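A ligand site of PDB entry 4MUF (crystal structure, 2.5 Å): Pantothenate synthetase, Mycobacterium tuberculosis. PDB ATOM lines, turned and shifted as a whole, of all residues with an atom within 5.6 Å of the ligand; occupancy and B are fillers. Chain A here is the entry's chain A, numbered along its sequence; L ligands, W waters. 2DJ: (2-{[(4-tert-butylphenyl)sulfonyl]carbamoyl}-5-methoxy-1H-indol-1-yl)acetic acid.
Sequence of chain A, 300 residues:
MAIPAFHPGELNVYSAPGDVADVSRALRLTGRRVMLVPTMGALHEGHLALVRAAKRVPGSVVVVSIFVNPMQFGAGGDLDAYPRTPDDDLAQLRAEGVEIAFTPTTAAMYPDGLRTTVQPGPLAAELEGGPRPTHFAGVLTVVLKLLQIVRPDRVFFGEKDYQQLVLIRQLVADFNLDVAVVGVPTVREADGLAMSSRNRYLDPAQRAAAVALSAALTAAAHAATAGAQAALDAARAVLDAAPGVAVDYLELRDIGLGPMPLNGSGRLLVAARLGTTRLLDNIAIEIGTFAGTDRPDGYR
An oxygen (OXT) of the ligand lies within hydrogen-bond range of the backbone NH of Ser 197 (3.5 Å).
The side-chain hydroxyl (OG) of Ser 196 sits at hydrogen-bond distance from an oxygen (O) of the ligand, 3.3 Å away.
OAG of the ligand is in hydrogen-bond range of N of Met 40 (2.7 Å).
A ring nitrogen (NE2) of His 47 is in hydrogen-bond range of a nitrogen (NAS) of the ligand, at 2.9 Å.
The side-chain hydroxyl of Tyr 82 is in hydrogen-bond range of an oxygen (OAH) of the ligand (3.2 Å).
An oxygen (OAT) of the ligand lies within hydrogen-bond range of the backbone NH of Val 187.
The backbone NH (N) of Met 195 lies close to the backbone carbonyl oxygen (O) of Val 187 (3.2 Å).
The side-chain hydroxyl (OG) of Ser 196 is in hydrogen-bond range of the backbone NH (N) of Arg 198 (2.8 Å).
N of Gly 41 sits at hydrogen-bond distance from OG1 of Thr 39 (3.2 Å).
N of Val 184 is in hydrogen-bond range of O of Phe 157, at 2.7 Å.
The side-chain hydroxyl (OH) of Tyr 82 is in hydrogen-bond range of the side-chain hydroxyl (OG) of Ser 197, 3.1 Å away.
ND1 of His 47 lies within hydrogen-bond range of N of His 44 (2.9 Å).
N of Glu 159 sits at hydrogen-bond distance from O of Val 184 (2.8 Å).
N of Lys 160 lies within hydrogen-bond range of OG1 of Thr 186, 3.4 Å away.
The side-chain carboxylate (OD2) of Asp 161 lies close to an oxygen (OAF) of the ligand, at 3.1 Å.
Pro 38 touches the ligand (O to CAL, 3.3 Å).
CA of Thr 39 touches CAL of the ligand, at 3.5 Å.
Gly 41 touches the ligand (O to OAG, 3.9 Å).
His 44 touches the ligand.
Gly 46 touches the ligand (CA to OAT, 3.3 Å).
NE2 of Gln 72 touches CAD of the ligand (3.4 Å).
CG1 of Val 139 touches CAD of the ligand, 3.3 Å away.
Val 143 touches the ligand (CG2 to CAC, 3.6 Å).
CE1 of Phe 157 touches CAC of the ligand, 3.5 Å away.
CA of Gly 158 touches CAA of the ligand (3.6 Å).
Lys 160 touches the ligand.
Gln 164 touches the ligand (OE1 to CAK, 3.5 Å).
O of Val 184 touches CAA of the ligand, at 3.7 Å.
Pro 185 touches the ligand (O to CAA, 3.2 Å).
Thr 186 touches the ligand (CG2 to CAN, 3.9 Å).
Met 195 touches the ligand (O to CAO, 3.3 Å).
Hydrophobic or aromatic side chains that line the ligand: Met 40, His 44, His 47, Val 139, Val 143, Phe 157 and Val 187.
Within 4 Å of the ligand: Pro 38, Thr 39, Met 40, Gly 41, His 44, Gly 46, His 47, Gln 72, Tyr 82, Val 139, Val 143, Phe 157, Gly 158, Lys 160, Asp 161, Gln 164, Val 184, Pro 185, Thr 186, Val 187, Met 195, Ser 196 and Ser 197.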
ATOM      1  N   PRO A  38       2.167   3.752   9.820  1.00  0.00           N
ATOM      2  CA  PRO A  38       1.345   2.657   9.322  1.00  0.00           C
ATOM      3  C   PRO A  38       1.049   2.751   7.853  1.00  0.00           C
ATOM      4  O   PRO A  38       0.445   3.707   7.412  1.00  0.00           O
ATOM      5  CB  PRO A  38       0.054   2.753  10.128  1.00  0.00           C
ATOM      6  CG  PRO A  38       0.061   4.119  10.730  1.00  0.00           C
ATOM      7  CD  PRO A  38       1.500   4.465  10.936  1.00  0.00           C
ATOM      8  N   THR A  39       1.509   1.774   7.101  1.00  0.00           N
ATOM      9  CA  THR A  39       1.307   1.786   5.681  1.00  0.00           C
ATOM     10  C   THR A  39       0.569   0.539   5.235  1.00  0.00           C
ATOM     11  O   THR A  39       0.539  -0.494   5.961  1.00  0.00           O
ATOM     12  CB  THR A  39       2.641   1.952   4.930  1.00  0.00           C
ATOM     13  OG1 THR A  39       3.364   0.719   4.892  1.00  0.00           O
ATOM     14  CG2 THR A  39       3.487   3.009   5.604  1.00  0.00           C
ATOM     15  N   MET A  40      -0.051   0.665   4.069  1.00  0.00           N
ATOM     16  CA  MET A  40      -0.526  -0.470   3.291  1.00  0.00           C
ATOM     17  C   MET A  40       0.448  -0.754   2.149  1.00  0.00           C
ATOM     18  O   MET A  40       0.067  -1.241   1.093  1.00  0.00           O
ATOM     19  CB  MET A  40      -1.944  -0.234   2.752  1.00  0.00           C
ATOM     20  CG  MET A  40      -2.980  -0.197   3.813  1.00  0.00           C
ATOM     21  SD  MET A  40      -4.652  -0.555   3.207  1.00  0.00           S
ATOM     22  CE  MET A  40      -4.961   0.895   2.187  1.00  0.00           C
ATOM     23  N   GLY A  41       1.724  -0.481   2.391  1.00  0.00           N
ATOM     24  CA  GLY A  41       2.757  -0.788   1.392  1.00  0.00           C
ATOM     25  C   GLY A  41       2.662   0.105   0.168  1.00  0.00           C
ATOM     26  O   GLY A  41       1.999   1.177   0.186  1.00  0.00           O
ATOM     27  N   LEU A  43       5.060   1.913  -1.288  1.00  0.00           N
ATOM     28  CA  LEU A  43       5.512   3.145  -0.690  1.00  0.00           C
ATOM     29  C   LEU A  43       5.870   4.200  -1.712  1.00  0.00           C
ATOM     30  O   LEU A  43       6.431   3.900  -2.769  1.00  0.00           O
ATOM     31  CB  LEU A  43       6.673   2.875   0.273  1.00  0.00           C
ATOM     32  CG  LEU A  43       6.287   1.898   1.404  1.00  0.00           C
ATOM     33  CD1 LEU A  43       7.328   1.870   2.483  1.00  0.00           C
ATOM     34  CD2 LEU A  43       4.895   2.158   2.024  1.00  0.00           C
ATOM     35  N   HIS A  44       5.508   5.431  -1.415  1.00  0.00           N
ATOM     36  CA  HIS A  44       5.816   6.520  -2.311  1.00  0.00           C
ATOM     37  C   HIS A  44       6.492   7.658  -1.556  1.00  0.00           C
ATOM     38  O   HIS A  44       6.834   7.544  -0.374  1.00  0.00           O
ATOM     39  CB  HIS A  44       4.570   6.972  -3.052  1.00  0.00           C
ATOM     40  CG  HIS A  44       3.436   7.365  -2.164  1.00  0.00           C
ATOM     41  ND1 HIS A  44       2.216   6.726  -2.196  1.00  0.00           N
ATOM     42  CD2 HIS A  44       3.339   8.325  -1.219  1.00  0.00           C
ATOM     43  CE1 HIS A  44       1.410   7.283  -1.308  1.00  0.00           C
ATOM     44  NE2 HIS A  44       2.061   8.254  -0.700  1.00  0.00           N
ATOM     45  N   GLU A  45       6.671   8.777  -2.245  1.00  0.00           N
ATOM     46  CA  GLU A  45       7.357   9.933  -1.676  1.00  0.00           C
ATOM     47  C   GLU A  45       6.628  10.553  -0.430  1.00  0.00           C
ATOM     48  O   GLU A  45       7.234  11.320   0.363  1.00  0.00           O
ATOM     49  CB  GLU A  45       7.588  10.948  -2.807  1.00  0.00           C
ATOM     50  CG  GLU A  45       8.427  12.153  -2.486  1.00  0.00           C
ATOM     51  CD  GLU A  45       9.890  11.826  -2.189  1.00  0.00           C
ATOM     52  OE1 GLU A  45      10.454  10.874  -2.808  1.00  0.00           O
ATOM     53  OE2 GLU A  45      10.461  12.571  -1.334  1.00  0.00           O
ATOM     54  N   GLY A  46       5.360  10.202  -0.244  1.00  0.00           N
ATOM     55  CA  GLY A  46       4.579  10.665   0.914  1.00  0.00           C
ATOM     56  C   GLY A  46       4.914   9.816   2.125  1.00  0.00           C
ATOM     57  O   GLY A  46       5.092  10.300   3.246  1.00  0.00           O
ATOM     58  N   HIS A  47       5.034   8.518   1.864  1.00  0.00           N
ATOM     59  CA  HIS A  47       5.497   7.580   2.872  1.00  0.00           C
ATOM     60  C   HIS A  47       6.915   7.965   3.311  1.00  0.00           C
ATOM     61  O   HIS A  47       7.211   7.986   4.522  1.00  0.00           O
ATOM     62  CB  HIS A  47       5.422   6.161   2.340  1.00  0.00           C
ATOM     63  CG  HIS A  47       4.019   5.698   2.068  1.00  0.00           C
ATOM     64  ND1 HIS A  47       3.626   5.209   0.837  1.00  0.00           N
ATOM     65  CD2 HIS A  47       2.930   5.645   2.864  1.00  0.00           C
ATOM     66  CE1 HIS A  47       2.346   4.872   0.895  1.00  0.00           C
ATOM     67  NE2 HIS A  47       1.904   5.130   2.104  1.00  0.00           N
ATOM     68  N   ALA A  49       8.036  10.903   3.332  1.00  0.00           N
ATOM     69  CA  ALA A  49       7.838  12.090   4.195  1.00  0.00           C
ATOM     70  C   ALA A  49       7.471  11.722   5.627  1.00  0.00           C
ATOM     71  O   ALA A  49       8.101  12.179   6.576  1.00  0.00           O
ATOM     72  CB  ALA A  49       6.787  13.034   3.599  1.00  0.00           C
ATOM     73  N   LEU A  50       6.423  10.902   5.779  1.00  0.00           N
ATOM     74  CA  LEU A  50       6.038  10.319   7.071  1.00  0.00           C
ATOM     75  C   LEU A  50       7.248   9.800   7.860  1.00  0.00           C
ATOM     76  O   LEU A  50       7.437  10.194   9.022  1.00  0.00           O
ATOM     77  CB  LEU A  50       5.039   9.199   6.863  1.00  0.00           C
ATOM     78  CG  LEU A  50       3.741   9.519   6.094  1.00  0.00           C
ATOM     79  CD1 LEU A  50       2.821   8.305   6.151  1.00  0.00           C
ATOM     80  CD2 LEU A  50       3.014  10.768   6.625  1.00  0.00           C
ATOM     81  N   GLN A  72     -11.742  -3.240   4.917  1.00  0.00           N
ATOM     82  CA  GLN A  72     -12.155  -1.869   4.552  1.00  0.00           C
ATOM     83  C   GLN A  72     -12.351  -1.652   3.046  1.00  0.00           C
ATOM     84  O   GLN A  72     -12.959  -0.661   2.599  1.00  0.00           O
ATOM     85  CB  GLN A  72     -11.179  -0.838   5.150  1.00  0.00           C
ATOM     86  CG  GLN A  72      -9.765  -1.376   5.453  1.00  0.00           C
ATOM     87  CD  GLN A  72      -8.683  -0.316   5.394  1.00  0.00           C
ATOM     88  OE1 GLN A  72      -8.552   0.413   4.397  1.00  0.00           O
ATOM     89  NE2 GLN A  72      -7.876  -0.217   6.462  1.00  0.00           N
ATOM     90  N   TYR A  82      -5.396  -4.471  -4.534  1.00  0.00           N
ATOM     91  CA  TYR A  82      -4.287  -3.586  -4.129  1.00  0.00           C
ATOM     92  C   TYR A  82      -2.867  -3.953  -4.663  1.00  0.00           C
ATOM     93  O   TYR A  82      -2.555  -5.142  -4.821  1.00  0.00           O
ATOM     94  CB  TYR A  82      -4.273  -3.478  -2.596  1.00  0.00           C
ATOM     95  CG  TYR A  82      -3.841  -2.122  -2.094  1.00  0.00           C
ATOM     96  CD1 TYR A  82      -4.772  -1.101  -1.851  1.00  0.00           C
ATOM     97  CD2 TYR A  82      -2.498  -1.853  -1.854  1.00  0.00           C
ATOM     98  CE1 TYR A  82      -4.372   0.156  -1.390  1.00  0.00           C
ATOM     99  CE2 TYR A  82      -2.077  -0.605  -1.394  1.00  0.00           C
ATOM    100  CZ  TYR A  82      -3.020   0.390  -1.161  1.00  0.00           C
ATOM    101  OH  TYR A  82      -2.598   1.609  -0.707  1.00  0.00           O
ATOM    102  N   VAL A 139     -10.805   0.435   9.454  1.00  0.00           N
ATOM    103  CA  VAL A 139      -9.616   1.303   9.557  1.00  0.00           C
ATOM    104  C   VAL A 139      -9.296   1.515  11.017  1.00  0.00           C
ATOM    105  O   VAL A 139      -8.174   1.261  11.449  1.00  0.00           O
ATOM    106  CB  VAL A 139      -9.877   2.652   8.830  1.00  0.00           C
ATOM    107  CG1 VAL A 139      -8.661   3.563   8.899  1.00  0.00           C
ATOM    108  CG2 VAL A 139     -10.236   2.393   7.388  1.00  0.00           C
ATOM    109  N   VAL A 142      -8.059  -1.729  12.803  1.00  0.00           N
ATOM    110  CA  VAL A 142      -6.724  -2.256  12.582  1.00  0.00           C
ATOM    111  C   VAL A 142      -5.692  -1.235  13.056  1.00  0.00           C
ATOM    112  O   VAL A 142      -4.621  -1.613  13.537  1.00  0.00           O
ATOM    113  CB  VAL A 142      -6.490  -2.792  11.143  1.00  0.00           C
ATOM    114  CG1 VAL A 142      -6.519  -1.688  10.167  1.00  0.00           C
ATOM    115  CG2 VAL A 142      -5.162  -3.537  11.026  1.00  0.00           C
ATOM    116  N   VAL A 143      -6.027   0.042  12.957  1.00  0.00           N
ATOM    117  CA  VAL A 143      -5.163   1.078  13.528  1.00  0.00           C
ATOM    118  C   VAL A 143      -4.992   0.810  15.015  1.00  0.00           C
ATOM    119  O   VAL A 143      -3.884   0.884  15.531  1.00  0.00           O
ATOM    120  CB  VAL A 143      -5.706   2.519  13.253  1.00  0.00           C
ATOM    121  CG1 VAL A 143      -5.019   3.540  14.150  1.00  0.00           C
ATOM    122  CG2 VAL A 143      -5.437   2.887  11.797  1.00  0.00           C
ATOM    123  N   LEU A 146      -2.853  -1.988  15.711  1.00  0.00           N
ATOM    124  CA  LEU A 146      -1.495  -1.594  15.412  1.00  0.00           C
ATOM    125  C   LEU A 146      -0.857  -0.685  16.460  1.00  0.00           C
ATOM    126  O   LEU A 146       0.344  -0.777  16.702  1.00  0.00           O
ATOM    127  CB  LEU A 146      -1.470  -0.899  14.086  1.00  0.00           C
ATOM    128  CG  LEU A 146      -1.546  -1.836  12.880  1.00  0.00           C
ATOM    129  CD1 LEU A 146      -1.732  -0.914  11.725  1.00  0.00           C
ATOM    130  CD2 LEU A 146      -0.278  -2.731  12.721  1.00  0.00           C
ATOM    131  N   PHE A 157       0.444  10.101   9.987  1.00  0.00           N
ATOM    132  CA  PHE A 157      -0.423   9.990   8.839  1.00  0.00           C
ATOM    133  C   PHE A 157      -0.217  11.144   7.879  1.00  0.00           C
ATOM    134  O   PHE A 157       0.126  12.245   8.310  1.00  0.00           O
ATOM    135  CB  PHE A 157      -1.870   9.916   9.340  1.00  0.00           C
ATOM    136  CG  PHE A 157      -2.159   8.706  10.172  1.00  0.00           C
ATOM    137  CD1 PHE A 157      -2.184   7.439   9.598  1.00  0.00           C
ATOM    138  CD2 PHE A 157      -2.416   8.829  11.528  1.00  0.00           C
ATOM    139  CE1 PHE A 157      -2.462   6.302  10.375  1.00  0.00           C
ATOM    140  CE2 PHE A 157      -2.696   7.721  12.311  1.00  0.00           C
ATOM    141  CZ  PHE A 157      -2.701   6.453  11.747  1.00  0.00           C
ATOM    142  N   GLY A 158      -0.393  10.911   6.582  1.00  0.00           N
ATOM    143  CA  GLY A 158      -0.436  12.004   5.621  1.00  0.00           C
ATOM    144  C   GLY A 158      -1.773  12.690   5.774  1.00  0.00           C
ATOM    145  O   GLY A 158      -2.649  12.163   6.463  1.00  0.00           O
ATOM    146  N   GLU A 159      -1.953  13.859   5.174  1.00  0.00           N
ATOM    147  CA  GLU A 159      -3.244  14.565   5.310  1.00  0.00           C
ATOM    148  C   GLU A 159      -4.239  14.301   4.150  1.00  0.00           C
ATOM    149  O   GLU A 159      -5.364  14.813   4.158  1.00  0.00           O
ATOM    150  CB  GLU A 159      -3.046  16.073   5.541  1.00  0.00           C
ATOM    151  CG  GLU A 159      -2.625  16.429   6.959  1.00  0.00           C
ATOM    152  CD  GLU A 159      -2.191  17.900   7.162  1.00  0.00           C
ATOM    153  OE1 GLU A 159      -2.247  18.688   6.199  1.00  0.00           O
ATOM    154  OE2 GLU A 159      -1.805  18.265   8.286  1.00  0.00           O
ATOM    155  N   LYS A 160      -3.818  13.488   3.174  1.00  0.00           N
ATOM    156  CA  LYS A 160      -4.631  13.229   1.980  1.00  0.00           C
ATOM    157  C   LYS A 160      -5.980  12.755   2.439  1.00  0.00           C
ATOM    158  O   LYS A 160      -6.999  13.366   2.132  1.00  0.00           O
ATOM    159  CB  LYS A 160      -4.000  12.153   1.057  1.00  0.00           C
ATOM    160  CG  LYS A 160      -4.370  12.285  -0.440  1.00  0.00           C
ATOM    161  CD  LYS A 160      -4.708  10.928  -1.127  1.00  0.00           C
ATOM    162  CE  LYS A 160      -4.676  11.089  -2.676  1.00  0.00           C
ATOM    163  NZ  LYS A 160      -5.851  10.601  -3.572  1.00  0.00           N
ATOM    164  N   ASP A 161      -5.954  11.681   3.237  1.00  0.00           N
ATOM    165  CA  ASP A 161      -7.142  11.033   3.741  1.00  0.00           C
ATOM    166  C   ASP A 161      -7.519  11.708   5.050  1.00  0.00           C
ATOM    167  O   ASP A 161      -7.229  11.239   6.144  1.00  0.00           O
ATOM    168  CB  ASP A 161      -6.917   9.521   3.848  1.00  0.00           C
ATOM    169  CG  ASP A 161      -6.393   8.923   2.541  1.00  0.00           C
ATOM    170  OD1 ASP A 161      -7.118   8.989   1.533  1.00  0.00           O
ATOM    171  OD2 ASP A 161      -5.236   8.398   2.510  1.00  0.00           O
ATOM    172  N   GLN A 164     -10.321  10.188   7.647  1.00  0.00           N
ATOM    173  CA  GLN A 164      -9.549   9.146   8.304  1.00  0.00           C
ATOM    174  C   GLN A 164      -8.648   9.669   9.420  1.00  0.00           C
ATOM    175  O   GLN A 164      -8.586   9.055  10.490  1.00  0.00           O
ATOM    176  CB  GLN A 164      -8.704   8.440   7.236  1.00  0.00           C
ATOM    177  CG  GLN A 164      -7.504   7.675   7.778  1.00  0.00           C
ATOM    178  CD  GLN A 164      -6.822   6.857   6.703  1.00  0.00           C
ATOM    179  OE1 GLN A 164      -7.346   5.852   6.226  1.00  0.00           O
ATOM    180  NE2 GLN A 164      -5.621   7.285   6.314  1.00  0.00           N
ATOM    181  N   ILE A 168      -9.172   8.949  13.370  1.00  0.00           N
ATOM    182  CA  ILE A 168      -8.103   8.459  14.215  1.00  0.00           C
ATOM    183  C   ILE A 168      -7.869   9.387  15.410  1.00  0.00           C
ATOM    184  O   ILE A 168      -7.692   8.916  16.507  1.00  0.00           O
ATOM    185  CB  ILE A 168      -6.784   8.223  13.424  1.00  0.00           C
ATOM    186  CG1 ILE A 168      -6.910   7.012  12.507  1.00  0.00           C
ATOM    187  CG2 ILE A 168      -5.590   7.977  14.366  1.00  0.00           C
ATOM    188  CD1 ILE A 168      -5.998   7.082  11.295  1.00  0.00           C
ATOM    189  N   VAL A 184       0.641  14.929   8.588  1.00  0.00           N
ATOM    190  CA  VAL A 184       1.713  15.415   7.718  1.00  0.00           C
ATOM    191  C   VAL A 184       1.143  15.931   6.393  1.00  0.00           C
ATOM    192  O   VAL A 184       0.376  15.226   5.719  1.00  0.00           O
ATOM    193  CB  VAL A 184       2.766  14.340   7.467  1.00  0.00           C
ATOM    194  CG1 VAL A 184       3.960  14.908   6.713  1.00  0.00           C
ATOM    195  CG2 VAL A 184       3.189  13.739   8.778  1.00  0.00           C
ATOM    196  N   PRO A 185       1.529  17.170   6.019  1.00  0.00           N
ATOM    197  CA  PRO A 185       1.005  17.783   4.803  1.00  0.00           C
ATOM    198  C   PRO A 185       1.181  16.901   3.570  1.00  0.00           C
ATOM    199  O   PRO A 185       2.248  16.300   3.355  1.00  0.00           O
ATOM    200  CB  PRO A 185       1.829  19.064   4.689  1.00  0.00           C
ATOM    201  CG  PRO A 185       2.186  19.410   6.109  1.00  0.00           C
ATOM    202  CD  PRO A 185       2.482  18.059   6.714  1.00  0.00           C
ATOM    203  N   THR A 186       0.130  16.796   2.776  1.00  0.00           N
ATOM    204  CA  THR A 186       0.199  15.974   1.591  1.00  0.00           C
ATOM    205  C   THR A 186       1.408  16.403   0.741  1.00  0.00           C
ATOM    206  O   THR A 186       1.649  17.592   0.515  1.00  0.00           O
ATOM    207  CB  THR A 186      -1.036  16.117   0.737  1.00  0.00           C
ATOM    208  OG1 THR A 186      -2.193  15.987   1.543  1.00  0.00           O
ATOM    209  CG2 THR A 186      -1.057  15.054  -0.335  1.00  0.00           C
ATOM    210  N   VAL A 187       2.147  15.388   0.297  1.00  0.00           N
ATOM    211  CA  VAL A 187       3.237  15.517  -0.638  1.00  0.00           C
ATOM    212  C   VAL A 187       2.603  15.302  -2.008  1.00  0.00           C
ATOM    213  O   VAL A 187       1.857  14.363  -2.197  1.00  0.00           O
ATOM    214  CB  VAL A 187       4.307  14.429  -0.328  1.00  0.00           C
ATOM    215  CG1 VAL A 187       5.373  14.303  -1.455  1.00  0.00           C
ATOM    216  CG2 VAL A 187       4.944  14.696   1.026  1.00  0.00           C
ATOM    217  N   MET A 195      -0.293  12.746  -3.972  1.00  0.00           N
ATOM    218  CA  MET A 195       0.266  11.378  -4.077  1.00  0.00           C
ATOM    219  C   MET A 195      -0.741  10.299  -3.650  1.00  0.00           C
ATOM    220  O   MET A 195      -1.471  10.440  -2.662  1.00  0.00           O
ATOM    221  CB  MET A 195       1.539  11.215  -3.250  1.00  0.00           C
ATOM    222  CG  MET A 195       2.695  12.009  -3.739  1.00  0.00           C
ATOM    223  SD  MET A 195       3.577  11.330  -5.165  1.00  0.00           S
ATOM    224  CE  MET A 195       5.041  12.419  -5.085  1.00  0.00           C
ATOM    225  N   SER A 196      -0.774   9.229  -4.416  1.00  0.00           N
ATOM    226  CA  SER A 196      -1.758   8.201  -4.196  1.00  0.00           C
ATOM    227  C   SER A 196      -1.304   6.951  -4.911  1.00  0.00           C
ATOM    228  O   SER A 196      -0.704   7.014  -5.977  1.00  0.00           O
ATOM    229  CB  SER A 196      -3.130   8.634  -4.706  1.00  0.00           C
ATOM    230  OG  SER A 196      -4.053   7.555  -4.776  1.00  0.00           O
ATOM    231  N   SER A 197      -1.600   5.820  -4.280  1.00  0.00           N
ATOM    232  CA  SER A 197      -1.346   4.533  -4.884  1.00  0.00           C
ATOM    233  C   SER A 197      -2.271   4.398  -6.070  1.00  0.00           C
ATOM    234  O   SER A 197      -1.941   3.757  -7.069  1.00  0.00           O
ATOM    235  CB  SER A 197      -1.618   3.399  -3.873  1.00  0.00           C
ATOM    236  OG  SER A 197      -2.662   3.737  -2.954  1.00  0.00           O
ATOM    237  N   ARG A 198      -3.418   5.068  -5.979  1.00  0.00           N
ATOM    238  CA  ARG A 198      -4.399   5.009  -7.058  1.00  0.00           C
ATOM    239  C   ARG A 198      -3.979   5.740  -8.366  1.00  0.00           C
ATOM    240  O   ARG A 198      -4.600   5.547  -9.405  1.00  0.00           O
ATOM    241  CB  ARG A 198      -5.760   5.480  -6.560  1.00  0.00           C
ATOM    242  CG  ARG A 198      -6.467   4.410  -5.735  1.00  0.00           C
ATOM    243  CD  ARG A 198      -7.751   4.964  -5.151  1.00  0.00           C
ATOM    244  NE  ARG A 198      -8.658   3.915  -4.670  1.00  0.00           N
ATOM    245  CZ  ARG A 198      -9.826   4.157  -4.074  1.00  0.00           C
ATOM    246  NH1 ARG A 198     -10.252   5.418  -3.893  1.00  0.00           N
ATOM    247  NH2 ARG A 198     -10.594   3.144  -3.665  1.00  0.00           N
HETATM  248  O   2DJ L   1      -3.554   6.894  -1.554  1.00  0.00           O
HETATM  249  C   2DJ L   1      -2.513   7.190  -0.881  1.00  0.00           C
HETATM  250  OXT 2DJ L   1      -1.401   6.622  -0.930  1.00  0.00           O
HETATM  251  CA  2DJ L   1      -2.593   8.395   0.011  1.00  0.00           C
HETATM  252  N   2DJ L   1      -1.515   8.473   1.084  1.00  0.00           N
HETATM  253  CBB 2DJ L   1      -0.683   9.515   1.214  1.00  0.00           C
HETATM  254  CAO 2DJ L   1      -0.582  10.633   0.472  1.00  0.00           C
HETATM  255  CAN 2DJ L   1       0.362  11.616   0.763  1.00  0.00           C
HETATM  256  CAW 2DJ L   1       1.193  11.443   1.870  1.00  0.00           C
HETATM  257  OAT 2DJ L   1       2.119  12.427   2.110  1.00  0.00           O
HETATM  258  CAA 2DJ L   1       2.166  13.056   3.382  1.00  0.00           C
HETATM  259  CAP 2DJ L   1       1.068  10.238   2.616  1.00  0.00           C
HETATM  260  CBA 2DJ L   1       0.131   9.321   2.275  1.00  0.00           C
HETATM  261  CAQ 2DJ L   1      -0.190   8.136   2.821  1.00  0.00           C
HETATM  262  CAZ 2DJ L   1      -1.216   7.637   2.109  1.00  0.00           C
HETATM  263  CAV 2DJ L   1      -1.800   6.455   2.301  1.00  0.00           C
HETATM  264  OAF 2DJ L   1      -3.006   6.268   2.085  1.00  0.00           O
HETATM  265  NAS 2DJ L   1      -0.947   5.467   2.569  1.00  0.00           N
HETATM  266  SBE 2DJ L   1      -1.614   3.994   2.654  1.00  0.00           S
HETATM  267  OAG 2DJ L   1      -0.521   2.897   2.536  1.00  0.00           O
HETATM  268  OAH 2DJ L   1      -2.635   3.935   1.489  1.00  0.00           O
HETATM  269  CAY 2DJ L   1      -2.542   3.749   4.058  1.00  0.00           C
HETATM  270  CAL 2DJ L   1      -1.900   3.119   5.100  1.00  0.00           C
HETATM  271  CAJ 2DJ L   1      -2.586   2.837   6.258  1.00  0.00           C
HETATM  272  CAX 2DJ L   1      -3.922   3.199   6.390  1.00  0.00           C
HETATM  273  CBD 2DJ L   1      -4.483   2.881   7.612  1.00  0.00           C
HETATM  274  CAC 2DJ L   1      -4.527   4.111   8.507  1.00  0.00           C
HETATM  275  CAD 2DJ L   1      -5.901   2.344   7.453  1.00  0.00           C
HETATM  276  CAB 2DJ L   1      -3.594   1.782   8.212  1.00  0.00           C
HETATM  277  CAK 2DJ L   1      -4.593   3.843   5.330  1.00  0.00           C
HETATM  278  CAM 2DJ L   1      -3.902   4.118   4.143  1.00  0.00           C
HETATM  279  O   HOH W   1      -1.915   7.963   5.848  1.00  0.00           O
